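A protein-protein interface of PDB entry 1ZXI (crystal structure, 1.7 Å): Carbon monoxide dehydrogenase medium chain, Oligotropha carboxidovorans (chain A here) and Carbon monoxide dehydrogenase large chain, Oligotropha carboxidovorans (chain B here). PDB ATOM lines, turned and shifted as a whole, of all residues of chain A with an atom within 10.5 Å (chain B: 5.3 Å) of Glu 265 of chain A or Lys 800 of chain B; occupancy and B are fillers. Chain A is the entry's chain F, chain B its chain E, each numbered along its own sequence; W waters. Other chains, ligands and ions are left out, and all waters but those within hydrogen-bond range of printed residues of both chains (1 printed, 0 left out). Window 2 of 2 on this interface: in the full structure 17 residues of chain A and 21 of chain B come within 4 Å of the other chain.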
ATOM      1  N   LEU A 186       3.250 -18.285   5.834  1.00  0.00           N
ATOM      2  CA  LEU A 186       1.805 -18.051   5.700  1.00  0.00           C
ATOM      3  C   LEU A 186       1.168 -19.414   5.994  1.00  0.00           C
ATOM      4  O   LEU A 186       1.535 -20.401   5.368  1.00  0.00           O
ATOM      5  CB  LEU A 186       1.453 -17.605   4.279  1.00  0.00           C
ATOM      6  CG  LEU A 186      -0.038 -17.389   3.995  1.00  0.00           C
ATOM      7  CD1 LEU A 186      -0.546 -16.241   4.859  1.00  0.00           C
ATOM      8  CD2 LEU A 186      -0.275 -17.091   2.532  1.00  0.00           C
ATOM      9  N   THR A 195       1.320 -22.617   3.781  1.00  0.00           N
ATOM     10  CA  THR A 195       0.625 -22.431   2.519  1.00  0.00           C
ATOM     11  C   THR A 195       1.820 -22.098   1.591  1.00  0.00           C
ATOM     12  O   THR A 195       1.883 -22.523   0.434  1.00  0.00           O
ATOM     13  CB  THR A 195      -0.325 -21.233   2.637  1.00  0.00           C
ATOM     14  OG1 THR A 195      -1.397 -21.583   3.529  1.00  0.00           O
ATOM     15  CG2 THR A 195      -0.879 -20.833   1.259  1.00  0.00           C
ATOM     16  N   ALA A 196       2.754 -21.323   2.140  1.00  0.00           N
ATOM     17  CA  ALA A 196       4.018 -20.945   1.481  1.00  0.00           C
ATOM     18  C   ALA A 196       4.873 -20.245   2.533  1.00  0.00           C
ATOM     19  O   ALA A 196       4.326 -19.578   3.407  1.00  0.00           O
ATOM     20  CB  ALA A 196       3.766 -19.996   0.299  1.00  0.00           C
ATOM     21  N   ASN A 218       7.277 -25.730   1.188  1.00  0.00           N
ATOM     22  CA  ASN A 218       5.982 -26.310   0.833  1.00  0.00           C
ATOM     23  C   ASN A 218       5.289 -25.786  -0.425  1.00  0.00           C
ATOM     24  O   ASN A 218       4.063 -25.735  -0.485  1.00  0.00           O
ATOM     25  CB  ASN A 218       5.035 -26.222   2.058  1.00  0.00           C
ATOM     26  CG  ASN A 218       4.092 -27.406   2.148  1.00  0.00           C
ATOM     27  OD1 ASN A 218       4.338 -28.442   1.529  1.00  0.00           O
ATOM     28  ND2 ASN A 218       3.012 -27.268   2.924  1.00  0.00           N
ATOM     29  N   VAL A 219       6.077 -25.421  -1.436  1.00  0.00           N
ATOM     30  CA  VAL A 219       5.515 -24.937  -2.698  1.00  0.00           C
ATOM     31  C   VAL A 219       6.013 -25.779  -3.888  1.00  0.00           C
ATOM     32  O   VAL A 219       6.114 -25.303  -5.022  1.00  0.00           O
ATOM     33  CB  VAL A 219       5.790 -23.423  -2.907  1.00  0.00           C
ATOM     34  CG1 VAL A 219       4.937 -22.645  -1.925  1.00  0.00           C
ATOM     35  CG2 VAL A 219       7.271 -23.078  -2.683  1.00  0.00           C
ATOM     36  N   VAL A 247      11.164 -12.216  -7.311  1.00  0.00           N
ATOM     37  CA  VAL A 247       9.871 -12.899  -7.200  1.00  0.00           C
ATOM     38  C   VAL A 247       9.557 -13.720  -8.460  1.00  0.00           C
ATOM     39  O   VAL A 247       9.045 -14.833  -8.378  1.00  0.00           O
ATOM     40  CB  VAL A 247       8.724 -11.862  -6.925  1.00  0.00           C
ATOM     41  CG1 VAL A 247       7.347 -12.518  -7.114  1.00  0.00           C
ATOM     42  CG2 VAL A 247       8.880 -11.307  -5.512  1.00  0.00           C
ATOM     43  N   GLU A 251       8.997 -17.739  -8.153  1.00  0.00           N
ATOM     44  CA  GLU A 251       7.702 -18.284  -8.546  1.00  0.00           C
ATOM     45  C   GLU A 251       7.888 -19.297  -9.671  1.00  0.00           C
ATOM     46  O   GLU A 251       7.218 -20.335  -9.717  1.00  0.00           O
ATOM     47  CB  GLU A 251       6.776 -17.166  -9.035  1.00  0.00           C
ATOM     48  CG  GLU A 251       6.306 -16.189  -7.961  1.00  0.00           C
ATOM     49  CD  GLU A 251       5.377 -15.119  -8.535  1.00  0.00           C
ATOM     50  OE1 GLU A 251       5.367 -14.944  -9.774  1.00  0.00           O
ATOM     51  OE2 GLU A 251       4.679 -14.439  -7.754  1.00  0.00           O
ATOM     52  N   ALA A 252       8.807 -18.982 -10.582  1.00  0.00           N
ATOM     53  CA  ALA A 252       9.078 -19.834 -11.732  1.00  0.00           C
ATOM     54  C   ALA A 252       9.431 -21.276 -11.416  1.00  0.00           C
ATOM     55  O   ALA A 252       9.104 -22.169 -12.211  1.00  0.00           O
ATOM     56  CB  ALA A 252      10.183 -19.219 -12.581  1.00  0.00           C
ATOM     57  N   THR A 254       8.434 -22.956  -8.568  1.00  0.00           N
ATOM     58  CA  THR A 254       7.452 -23.593  -7.689  1.00  0.00           C
ATOM     59  C   THR A 254       6.523 -24.492  -8.503  1.00  0.00           C
ATOM     60  O   THR A 254       6.390 -24.325  -9.719  1.00  0.00           O
ATOM     61  CB  THR A 254       6.551 -22.542  -6.952  1.00  0.00           C
ATOM     62  OG1 THR A 254       5.810 -21.787  -7.918  1.00  0.00           O
ATOM     63  CG2 THR A 254       7.376 -21.601  -6.119  1.00  0.00           C
ATOM     64  N   ALA A 255       5.899 -25.454  -7.831  1.00  0.00           N
ATOM     65  CA  ALA A 255       4.933 -26.363  -8.454  1.00  0.00           C
ATOM     66  C   ALA A 255       4.156 -26.868  -7.242  1.00  0.00           C
ATOM     67  O   ALA A 255       4.236 -28.044  -6.892  1.00  0.00           O
ATOM     68  CB  ALA A 255       5.648 -27.516  -9.162  1.00  0.00           C
ATOM     69  N   PRO A 256       3.372 -25.982  -6.599  1.00  0.00           N
ATOM     70  CA  PRO A 256       2.615 -26.380  -5.408  1.00  0.00           C
ATOM     71  C   PRO A 256       1.502 -27.379  -5.598  1.00  0.00           C
ATOM     72  O   PRO A 256       1.033 -27.620  -6.703  1.00  0.00           O
ATOM     73  CB  PRO A 256       2.074 -25.047  -4.866  1.00  0.00           C
ATOM     74  CG  PRO A 256       2.899 -23.968  -5.587  1.00  0.00           C
ATOM     75  CD  PRO A 256       3.092 -24.578  -6.941  1.00  0.00           C
ATOM     76  N   ALA A 257       1.088 -27.978  -4.488  1.00  0.00           N
ATOM     77  CA  ALA A 257      -0.021 -28.908  -4.501  1.00  0.00           C
ATOM     78  C   ALA A 257      -1.273 -28.073  -4.301  1.00  0.00           C
ATOM     79  O   ALA A 257      -1.215 -27.004  -3.697  1.00  0.00           O
ATOM     80  CB  ALA A 257       0.116 -29.897  -3.354  1.00  0.00           C
ATOM     81  N   SER A 258      -2.400 -28.535  -4.822  1.00  0.00           N
ATOM     82  CA  SER A 258      -3.661 -27.828  -4.598  1.00  0.00           C
ATOM     83  C   SER A 258      -4.350 -28.625  -3.490  1.00  0.00           C
ATOM     84  O   SER A 258      -4.688 -29.800  -3.664  1.00  0.00           O
ATOM     85  CB  SER A 258      -4.517 -27.803  -5.867  1.00  0.00           C
ATOM     86  OG  SER A 258      -3.883 -27.016  -6.879  1.00  0.00           O
ATOM     87  N   ASP A 259      -4.503 -28.015  -2.323  1.00  0.00           N
ATOM     88  CA  ASP A 259      -5.143 -28.723  -1.224  1.00  0.00           C
ATOM     89  C   ASP A 259      -5.935 -27.760  -0.373  1.00  0.00           C
ATOM     90  O   ASP A 259      -6.347 -26.696  -0.860  1.00  0.00           O
ATOM     91  CB  ASP A 259      -4.106 -29.528  -0.391  1.00  0.00           C
ATOM     92  CG  ASP A 259      -2.996 -28.664   0.225  1.00  0.00           C
ATOM     93  OD1 ASP A 259      -3.232 -27.492   0.596  1.00  0.00           O
ATOM     94  OD2 ASP A 259      -1.871 -29.184   0.374  1.00  0.00           O
ATOM     95  N   ARG A 261      -5.105 -25.645   1.671  1.00  0.00           N
ATOM     96  CA  ARG A 261      -4.453 -24.348   1.779  1.00  0.00           C
ATOM     97  C   ARG A 261      -4.700 -23.486   0.540  1.00  0.00           C
ATOM     98  O   ARG A 261      -4.290 -22.329   0.494  1.00  0.00           O
ATOM     99  CB  ARG A 261      -2.943 -24.556   1.994  1.00  0.00           C
ATOM    100  CG  ARG A 261      -2.632 -25.336   3.284  1.00  0.00           C
ATOM    101  CD  ARG A 261      -1.161 -25.762   3.431  1.00  0.00           C
ATOM    102  NE  ARG A 261      -1.004 -26.651   4.582  1.00  0.00           N
ATOM    103  CZ  ARG A 261      -1.356 -27.936   4.614  1.00  0.00           C
ATOM    104  NH1 ARG A 261      -1.878 -28.540   3.542  1.00  0.00           N
ATOM    105  NH2 ARG A 261      -1.254 -28.617   5.750  1.00  0.00           N
ATOM    106  N   GLY A 262      -5.363 -24.058  -0.463  1.00  0.00           N
ATOM    107  CA  GLY A 262      -5.647 -23.308  -1.674  1.00  0.00           C
ATOM    108  C   GLY A 262      -5.044 -23.938  -2.926  1.00  0.00           C
ATOM    109  O   GLY A 262      -4.270 -24.902  -2.832  1.00  0.00           O
ATOM    110  N   PRO A 263      -5.396 -23.420  -4.112  1.00  0.00           N
ATOM    111  CA  PRO A 263      -4.886 -23.940  -5.396  1.00  0.00           C
ATOM    112  C   PRO A 263      -3.437 -23.551  -5.647  1.00  0.00           C
ATOM    113  O   PRO A 263      -2.921 -22.571  -5.085  1.00  0.00           O
ATOM    114  CB  PRO A 263      -5.827 -23.319  -6.430  1.00  0.00           C
ATOM    115  CG  PRO A 263      -6.162 -21.976  -5.808  1.00  0.00           C
ATOM    116  CD  PRO A 263      -6.368 -22.329  -4.326  1.00  0.00           C
ATOM    117  N   ALA A 264      -2.786 -24.320  -6.508  1.00  0.00           N
ATOM    118  CA  ALA A 264      -1.398 -24.090  -6.843  1.00  0.00           C
ATOM    119  C   ALA A 264      -1.086 -22.632  -7.195  1.00  0.00           C
ATOM    120  O   ALA A 264      -0.107 -22.073  -6.694  1.00  0.00           O
ATOM    121  CB  ALA A 264      -0.989 -25.018  -8.010  1.00  0.00           C
ATOM    122  N   GLU A 265      -1.914 -22.000  -8.027  1.00  0.00           N
ATOM    123  CA  GLU A 265      -1.609 -20.628  -8.422  1.00  0.00           C
ATOM    124  C   GLU A 265      -1.560 -19.675  -7.238  1.00  0.00           C
ATOM    125  O   GLU A 265      -0.740 -18.757  -7.220  1.00  0.00           O
ATOM    126  CB  GLU A 265      -2.582 -20.123  -9.504  1.00  0.00           C
ATOM    127  CG  GLU A 265      -4.035 -20.058  -9.089  1.00  0.00           C
ATOM    128  CD  GLU A 265      -4.757 -21.383  -9.252  1.00  0.00           C
ATOM    129  OE1 GLU A 265      -4.095 -22.436  -9.424  1.00  0.00           O
ATOM    130  OE2 GLU A 265      -6.007 -21.371  -9.195  1.00  0.00           O
ATOM    131  N   TYR A 266      -2.430 -19.884  -6.247  1.00  0.00           N
ATOM    132  CA  TYR A 266      -2.403 -19.041  -5.063  1.00  0.00           C
ATOM    133  C   TYR A 266      -1.102 -19.257  -4.291  1.00  0.00           C
ATOM    134  O   TYR A 266      -0.481 -18.288  -3.849  1.00  0.00           O
ATOM    135  CB  TYR A 266      -3.584 -19.379  -4.135  1.00  0.00           C
ATOM    136  CG  TYR A 266      -3.501 -18.703  -2.779  1.00  0.00           C
ATOM    137  CD1 TYR A 266      -3.468 -17.301  -2.681  1.00  0.00           C
ATOM    138  CD2 TYR A 266      -3.509 -19.453  -1.592  1.00  0.00           C
ATOM    139  CE1 TYR A 266      -3.448 -16.666  -1.454  1.00  0.00           C
ATOM    140  CE2 TYR A 266      -3.493 -18.822  -0.345  1.00  0.00           C
ATOM    141  CZ  TYR A 266      -3.466 -17.432  -0.286  1.00  0.00           C
ATOM    142  OH  TYR A 266      -3.490 -16.791   0.925  1.00  0.00           O
ATOM    143  N   ARG A 267      -0.693 -20.517  -4.128  1.00  0.00           N
ATOM    144  CA  ARG A 267       0.522 -20.822  -3.362  1.00  0.00           C
ATOM    145  C   ARG A 267       1.792 -20.314  -4.049  1.00  0.00           C
ATOM    146  O   ARG A 267       2.724 -19.859  -3.394  1.00  0.00           O
ATOM    147  CB  ARG A 267       0.585 -22.321  -3.068  1.00  0.00           C
ATOM    148  CG  ARG A 267      -0.689 -22.791  -2.377  1.00  0.00           C
ATOM    149  CD  ARG A 267      -0.642 -24.264  -2.036  1.00  0.00           C
ATOM    150  NE  ARG A 267       0.256 -24.549  -0.915  1.00  0.00           N
ATOM    151  CZ  ARG A 267       0.349 -25.755  -0.357  1.00  0.00           C
ATOM    152  NH1 ARG A 267      -0.382 -26.756  -0.833  1.00  0.00           N
ATOM    153  NH2 ARG A 267       1.106 -25.955   0.715  1.00  0.00           N
ATOM    154  N   THR A 268       1.805 -20.350  -5.371  1.00  0.00           N
ATOM    155  CA  THR A 268       2.953 -19.814  -6.099  1.00  0.00           C
ATOM    156  C   THR A 268       3.036 -18.293  -5.821  1.00  0.00           C
ATOM    157  O   THR A 268       4.097 -17.744  -5.514  1.00  0.00           O
ATOM    158  CB  THR A 268       2.772 -20.066  -7.599  1.00  0.00           C
ATOM    159  OG1 THR A 268       3.008 -21.460  -7.862  1.00  0.00           O
ATOM    160  CG2 THR A 268       3.715 -19.170  -8.417  1.00  0.00           C
ATOM    161  N   LYS A 269       1.900 -17.609  -5.938  1.00  0.00           N
ATOM    162  CA  LYS A 269       1.872 -16.180  -5.691  1.00  0.00           C
ATOM    163  C   LYS A 269       2.288 -15.896  -4.240  1.00  0.00           C
ATOM    164  O   LYS A 269       3.050 -14.956  -3.969  1.00  0.00           O
ATOM    165  CB  LYS A 269       0.464 -15.637  -5.969  1.00  0.00           C
ATOM    166  CG  LYS A 269       0.351 -14.129  -5.849  1.00  0.00           C
ATOM    167  CD  LYS A 269       1.084 -13.413  -7.007  1.00  0.00           C
ATOM    168  CE  LYS A 269       0.789 -11.907  -6.986  1.00  0.00           C
ATOM    169  NZ  LYS A 269       1.301 -11.202  -8.201  1.00  0.00           N
ATOM    170  N   MET A 270       1.819 -16.718  -3.302  1.00  0.00           N
ATOM    171  CA  MET A 270       2.187 -16.504  -1.903  1.00  0.00           C
ATOM    172  C   MET A 270       3.687 -16.756  -1.643  1.00  0.00           C
ATOM    173  O   MET A 270       4.275 -16.148  -0.752  1.00  0.00           O
ATOM    174  CB  MET A 270       1.319 -17.376  -0.985  1.00  0.00           C
ATOM    175  CG  MET A 270      -0.164 -16.924  -0.990  1.00  0.00           C
ATOM    176  SD  MET A 270      -0.395 -15.160  -0.577  1.00  0.00           S
ATOM    177  CE  MET A 270      -0.598 -14.416  -2.250  1.00  0.00           C
ATOM    178  N   ALA A 271       4.305 -17.653  -2.404  1.00  0.00           N
ATOM    179  CA  ALA A 271       5.739 -17.882  -2.222  1.00  0.00           C
ATOM    180  C   ALA A 271       6.423 -16.541  -2.550  1.00  0.00           C
ATOM    181  O   ALA A 271       7.373 -16.103  -1.874  1.00  0.00           O
ATOM    182  CB  ALA A 271       6.219 -18.979  -3.167  1.00  0.00           C
ATOM    183  N   GLY A 272       5.903 -15.873  -3.572  1.00  0.00           N
ATOM    184  CA  GLY A 272       6.442 -14.584  -3.954  1.00  0.00           C
ATOM    185  C   GLY A 272       6.211 -13.505  -2.905  1.00  0.00           C
ATOM    186  O   GLY A 272       7.111 -12.723  -2.619  1.00  0.00           O
ATOM    187  N   VAL A 273       5.013 -13.450  -2.318  1.00  0.00           N
ATOM    188  CA  VAL A 273       4.727 -12.429  -1.307  1.00  0.00           C
ATOM    189  C   VAL A 273       5.524 -12.677  -0.034  1.00  0.00           C
ATOM    190  O   VAL A 273       6.030 -11.739   0.601  1.00  0.00           O
ATOM    191  CB  VAL A 273       3.208 -12.372  -0.979  1.00  0.00           C
ATOM    192  CG1 VAL A 273       2.964 -11.383   0.152  1.00  0.00           C
ATOM    193  CG2 VAL A 273       2.413 -11.955  -2.253  1.00  0.00           C
ATOM    194  N   ALA B 795      -8.170 -17.296   3.580  1.00  0.00           N
ATOM    195  CA  ALA B 795      -7.264 -16.507   2.763  1.00  0.00           C
ATOM    196  C   ALA B 795      -7.214 -16.808   1.277  1.00  0.00           C
ATOM    197  O   ALA B 795      -7.199 -15.889   0.484  1.00  0.00           O
ATOM    198  CB  ALA B 795      -5.846 -16.540   3.371  1.00  0.00           C
ATOM    199  N   TRP B 796      -7.179 -18.073   0.879  1.00  0.00           N
ATOM    200  CA  TRP B 796      -7.125 -18.319  -0.553  1.00  0.00           C
ATOM    201  C   TRP B 796      -8.386 -17.841  -1.258  1.00  0.00           C
ATOM    202  O   TRP B 796      -8.311 -17.287  -2.358  1.00  0.00           O
ATOM    203  CB  TRP B 796      -6.844 -19.800  -0.873  1.00  0.00           C
ATOM    204  CG  TRP B 796      -7.973 -20.815  -0.736  1.00  0.00           C
ATOM    205  CD1 TRP B 796      -8.217 -21.641   0.335  1.00  0.00           C
ATOM    206  CD2 TRP B 796      -8.944 -21.170  -1.738  1.00  0.00           C
ATOM    207  NE1 TRP B 796      -9.266 -22.487   0.056  1.00  0.00           N
ATOM    208  CE2 TRP B 796      -9.733 -22.220  -1.205  1.00  0.00           C
ATOM    209  CE3 TRP B 796      -9.218 -20.707  -3.034  1.00  0.00           C
ATOM    210  CZ2 TRP B 796     -10.788 -22.818  -1.926  1.00  0.00           C
ATOM    211  CZ3 TRP B 796     -10.260 -21.303  -3.756  1.00  0.00           C
ATOM    212  CH2 TRP B 796     -11.033 -22.353  -3.193  1.00  0.00           C
ATOM    213  N   ARG B 797      -9.549 -18.014  -0.636  1.00  0.00           N
ATOM    214  CA  ARG B 797     -10.767 -17.544  -1.289  1.00  0.00           C
ATOM    215  C   ARG B 797     -10.860 -16.021  -1.375  1.00  0.00           C
ATOM    216  O   ARG B 797     -11.356 -15.500  -2.380  1.00  0.00           O
ATOM    217  CB  ARG B 797     -12.005 -18.151  -0.616  1.00  0.00           C
ATOM    218  CG  ARG B 797     -12.395 -19.485  -1.291  1.00  0.00           C
ATOM    219  CD  ARG B 797     -13.373 -20.348  -0.471  1.00  0.00           C
ATOM    220  NE  ARG B 797     -12.652 -21.047   0.585  1.00  0.00           N
ATOM    221  CZ  ARG B 797     -12.830 -22.315   0.936  1.00  0.00           C
ATOM    222  NH1 ARG B 797     -13.727 -23.089   0.323  1.00  0.00           N
ATOM    223  NH2 ARG B 797     -12.082 -22.812   1.913  1.00  0.00           N
ATOM    224  N   LEU B 798     -10.398 -15.295  -0.355  1.00  0.00           N
ATOM    225  CA  LEU B 798     -10.438 -13.829  -0.438  1.00  0.00           C
ATOM    226  C   LEU B 798      -9.350 -13.367  -1.420  1.00  0.00           C
ATOM    227  O   LEU B 798      -9.491 -12.314  -2.059  1.00  0.00           O
ATOM    228  CB  LEU B 798     -10.258 -13.160   0.941  1.00  0.00           C
ATOM    229  CG  LEU B 798     -11.407 -13.438   1.934  1.00  0.00           C
ATOM    230  CD1 LEU B 798     -11.264 -12.487   3.144  1.00  0.00           C
ATOM    231  CD2 LEU B 798     -12.771 -13.219   1.232  1.00  0.00           C
ATOM    232  N   TRP B 799      -8.279 -14.152  -1.559  1.00  0.00           N
ATOM    233  CA  TRP B 799      -7.248 -13.791  -2.537  1.00  0.00           C
ATOM    234  C   TRP B 799      -7.887 -13.869  -3.923  1.00  0.00           C
ATOM    235  O   TRP B 799      -7.667 -12.990  -4.765  1.00  0.00           O
ATOM    236  CB  TRP B 799      -6.056 -14.741  -2.489  1.00  0.00           C
ATOM    237  CG  TRP B 799      -5.021 -14.439  -3.564  1.00  0.00           C
ATOM    238  CD1 TRP B 799      -4.034 -13.500  -3.510  1.00  0.00           C
ATOM    239  CD2 TRP B 799      -4.871 -15.111  -4.817  1.00  0.00           C
ATOM    240  NE1 TRP B 799      -3.261 -13.550  -4.655  1.00  0.00           N
ATOM    241  CE2 TRP B 799      -3.753 -14.531  -5.473  1.00  0.00           C
ATOM    242  CE3 TRP B 799      -5.568 -16.147  -5.452  1.00  0.00           C
ATOM    243  CZ2 TRP B 799      -3.314 -14.958  -6.733  1.00  0.00           C
ATOM    244  CZ3 TRP B 799      -5.131 -16.576  -6.714  1.00  0.00           C
ATOM    245  CH2 TRP B 799      -4.016 -15.981  -7.333  1.00  0.00           C
ATOM    246  N   LYS B 800      -8.680 -14.919  -4.150  1.00  0.00           N
ATOM    247  CA  LYS B 800      -9.358 -15.119  -5.440  1.00  0.00           C
ATOM    248  C   LYS B 800     -10.326 -13.958  -5.726  1.00  0.00           C
ATOM    249  O   LYS B 800     -10.475 -13.530  -6.877  1.00  0.00           O
ATOM    250  CB  LYS B 800     -10.138 -16.455  -5.447  1.00  0.00           C
ATOM    251  CG  LYS B 800      -9.284 -17.711  -5.645  1.00  0.00           C
ATOM    252  CD  LYS B 800      -8.760 -17.791  -7.071  1.00  0.00           C
ATOM    253  CE  LYS B 800      -7.982 -19.084  -7.329  1.00  0.00           C
ATOM    254  NZ  LYS B 800      -7.653 -19.168  -8.795  1.00  0.00           N
ATOM    255  N   VAL B 801     -10.995 -13.456  -4.693  1.00  0.00           N
ATOM    256  CA  VAL B 801     -11.896 -12.316  -4.890  1.00  0.00           C
ATOM    257  C   VAL B 801     -11.066 -11.142  -5.413  1.00  0.00           C
ATOM    258  O   VAL B 801     -11.420 -10.508  -6.413  1.00  0.00           O
ATOM    259  CB  VAL B 801     -12.594 -11.897  -3.559  1.00  0.00           C
ATOM    260  CG1 VAL B 801     -13.308 -10.564  -3.725  1.00  0.00           C
ATOM    261  CG2 VAL B 801     -13.582 -12.987  -3.131  1.00  0.00           C
ATOM    262  N   GLY B 802      -9.953 -10.854  -4.741  1.00  0.00           N
ATOM    263  CA  GLY B 802      -9.104  -9.754  -5.175  1.00  0.00           C
ATOM    264  C   GLY B 802      -8.509  -9.980  -6.559  1.00  0.00           C
ATOM    265  O   GLY B 802      -8.416  -9.050  -7.368  1.00  0.00           O
ATOM    266  N   GLU B 803      -8.103 -11.219  -6.820  1.00  0.00           N
ATOM    267  CA  GLU B 803      -7.527 -11.613  -8.097  1.00  0.00           C
ATOM    268  C   GLU B 803      -8.551 -11.310  -9.204  1.00  0.00           C
ATOM    269  O   GLU B 803      -8.226 -10.692 -10.212  1.00  0.00           O
ATOM    270  CB  GLU B 803      -7.183 -13.111  -8.027  1.00  0.00           C
ATOM    271  CG  GLU B 803      -6.468 -13.722  -9.210  1.00  0.00           C
ATOM    272  CD  GLU B 803      -5.153 -13.051  -9.571  1.00  0.00           C
ATOM    273  OE1 GLU B 803      -4.452 -12.460  -8.709  1.00  0.00           O
ATOM    274  OE2 GLU B 803      -4.820 -13.132 -10.767  1.00  0.00           O
ATOM    275  N   GLN B 804      -9.795 -11.713  -8.986  1.00  0.00           N
ATOM    276  CA  GLN B 804     -10.852 -11.492  -9.969  1.00  0.00           C
ATOM    277  C   GLN B 804     -11.313 -10.037 -10.126  1.00  0.00           C
ATOM    278  O   GLN B 804     -11.918  -9.680 -11.141  1.00  0.00           O
ATOM    279  CB  GLN B 804     -12.011 -12.436  -9.657  1.00  0.00           C
ATOM    280  CG  GLN B 804     -11.564 -13.887  -9.828  1.00  0.00           C
ATOM    281  CD  GLN B 804     -12.455 -14.903  -9.148  1.00  0.00           C
ATOM    282  OE1 GLN B 804     -12.091 -16.076  -9.042  1.00  0.00           O
ATOM    283  NE2 GLN B 804     -13.618 -14.469  -8.685  1.00  0.00           N
ATOM    284  N   LEU B 805     -10.998  -9.191  -9.150  1.00  0.00           N
ATOM    285  CA  LEU B 805     -11.332  -7.773  -9.224  1.00  0.00           C
ATOM    286  C   LEU B 805     -10.158  -6.983  -9.820  1.00  0.00           C
ATOM    287  O   LEU B 805     -10.206  -5.752  -9.899  1.00  0.00           O
ATOM    288  CB  LEU B 805     -11.638  -7.223  -7.835  1.00  0.00           C
ATOM    289  CG  LEU B 805     -12.950  -7.666  -7.190  1.00  0.00           C
ATOM    290  CD1 LEU B 805     -12.947  -7.182  -5.749  1.00  0.00           C
ATOM    291  CD2 LEU B 805     -14.153  -7.098  -7.961  1.00  0.00           C
HETATM  292  O   HOH W   1      -1.700 -12.508  -8.857  1.00  0.00           O
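Printed residues of chain B that touch a printed residue of chain A: Ala 795, Trp 796, Trp 799 and Lys 800. Of the 27 printed residues of chain A, 7 touch a printed residue of chain B. Hydrophobic or aromatic side chains of chain A that line the printed part of chain B: Pro 263, Tyr 266 and Met 270.
Among the printed residues, pairs that only touch across the chains: Arg 261 of chain A with Trp 796 of chain B (3.8 Å), Gly 262 of chain A with Trp 796 of chain B (3.5 Å), Pro 263 of chain A with Trp 796 of chain B (3.5 Å), Pro 263 of chain A with Lys 800 of chain B (3.7 Å), Tyr 266 of chain A with Ala 795 of chain B (3.4 Å), Tyr 266 of chain A with Trp 796 of chain B (3.4 Å), Tyr 266 of chain A with Trp 799 of chain B (3.4 Å), Lys 269 of chain A with Trp 799 of chain B (3.8 Å) and Met 270 of chain A with Trp 799 of chain B (3.7 Å).
Of chain B, only Lys 800 comes within 4 Å of Glu 265 of chain A. Lys 800 of chain B touches two residues of chain A. Of chain A, only Tyr 266 (3.4 Å), Lys 269 (3.8 Å) and Met 270 (3.7 Å) come within 4 Å of Trp 799 of chain B. No residue of chain A comes within 4 Å of Val 801 of chain B. No residue of chain A comes within 4 Å of Gln 804 of chain B. Of the printed residues of chain B, Lys 269 of chain A touches Trp 799 (3.8 Å). Of the printed residues of chain A, Trp 796 of chain B touches Arg 261 (3.8 Å), Gly 262 (3.5 Å), Pro 263 (3.5 Å) and Tyr 266 (3.4 Å). Printed residues of chain B within 4 Å of Arg 261 of chain A: Trp 796 (3.8 Å). Of the printed residues of chain B, Met 270 of chain A touches Trp 799. Of the printed residues of chain A, Ala 795 of chain B touches Tyr 266. Ser 258 of chain A touches none of the printed residues of chain B. Val 247 of chain A touches none of the printed residues of chain B. The nearest residue of chain B that does not touch Glu 265 of chain A is Trp 799 of chain B (4.3 Å). The nearest printed residue of chain B that does not touch Pro 263 of chain A is Trp 799 of chain B (5.6 Å).
The guanidinium group (NH1) of Arg 261 of chain A lies within salt-bridge range of the side-chain carboxylate (OD2) of Asp 259 of chain A (3.2 Å).
Water W1 lies within hydrogen-bond range of OE1 of Glu 803 of chain B (2.8 Å) and NZ of Lys 269 of chain A (3.3 Å).
The side-chain amino group of Lys 800 of chain B lies within salt-bridge range of the side-chain carboxylate of Glu 265 of chain A (2.8 Å).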
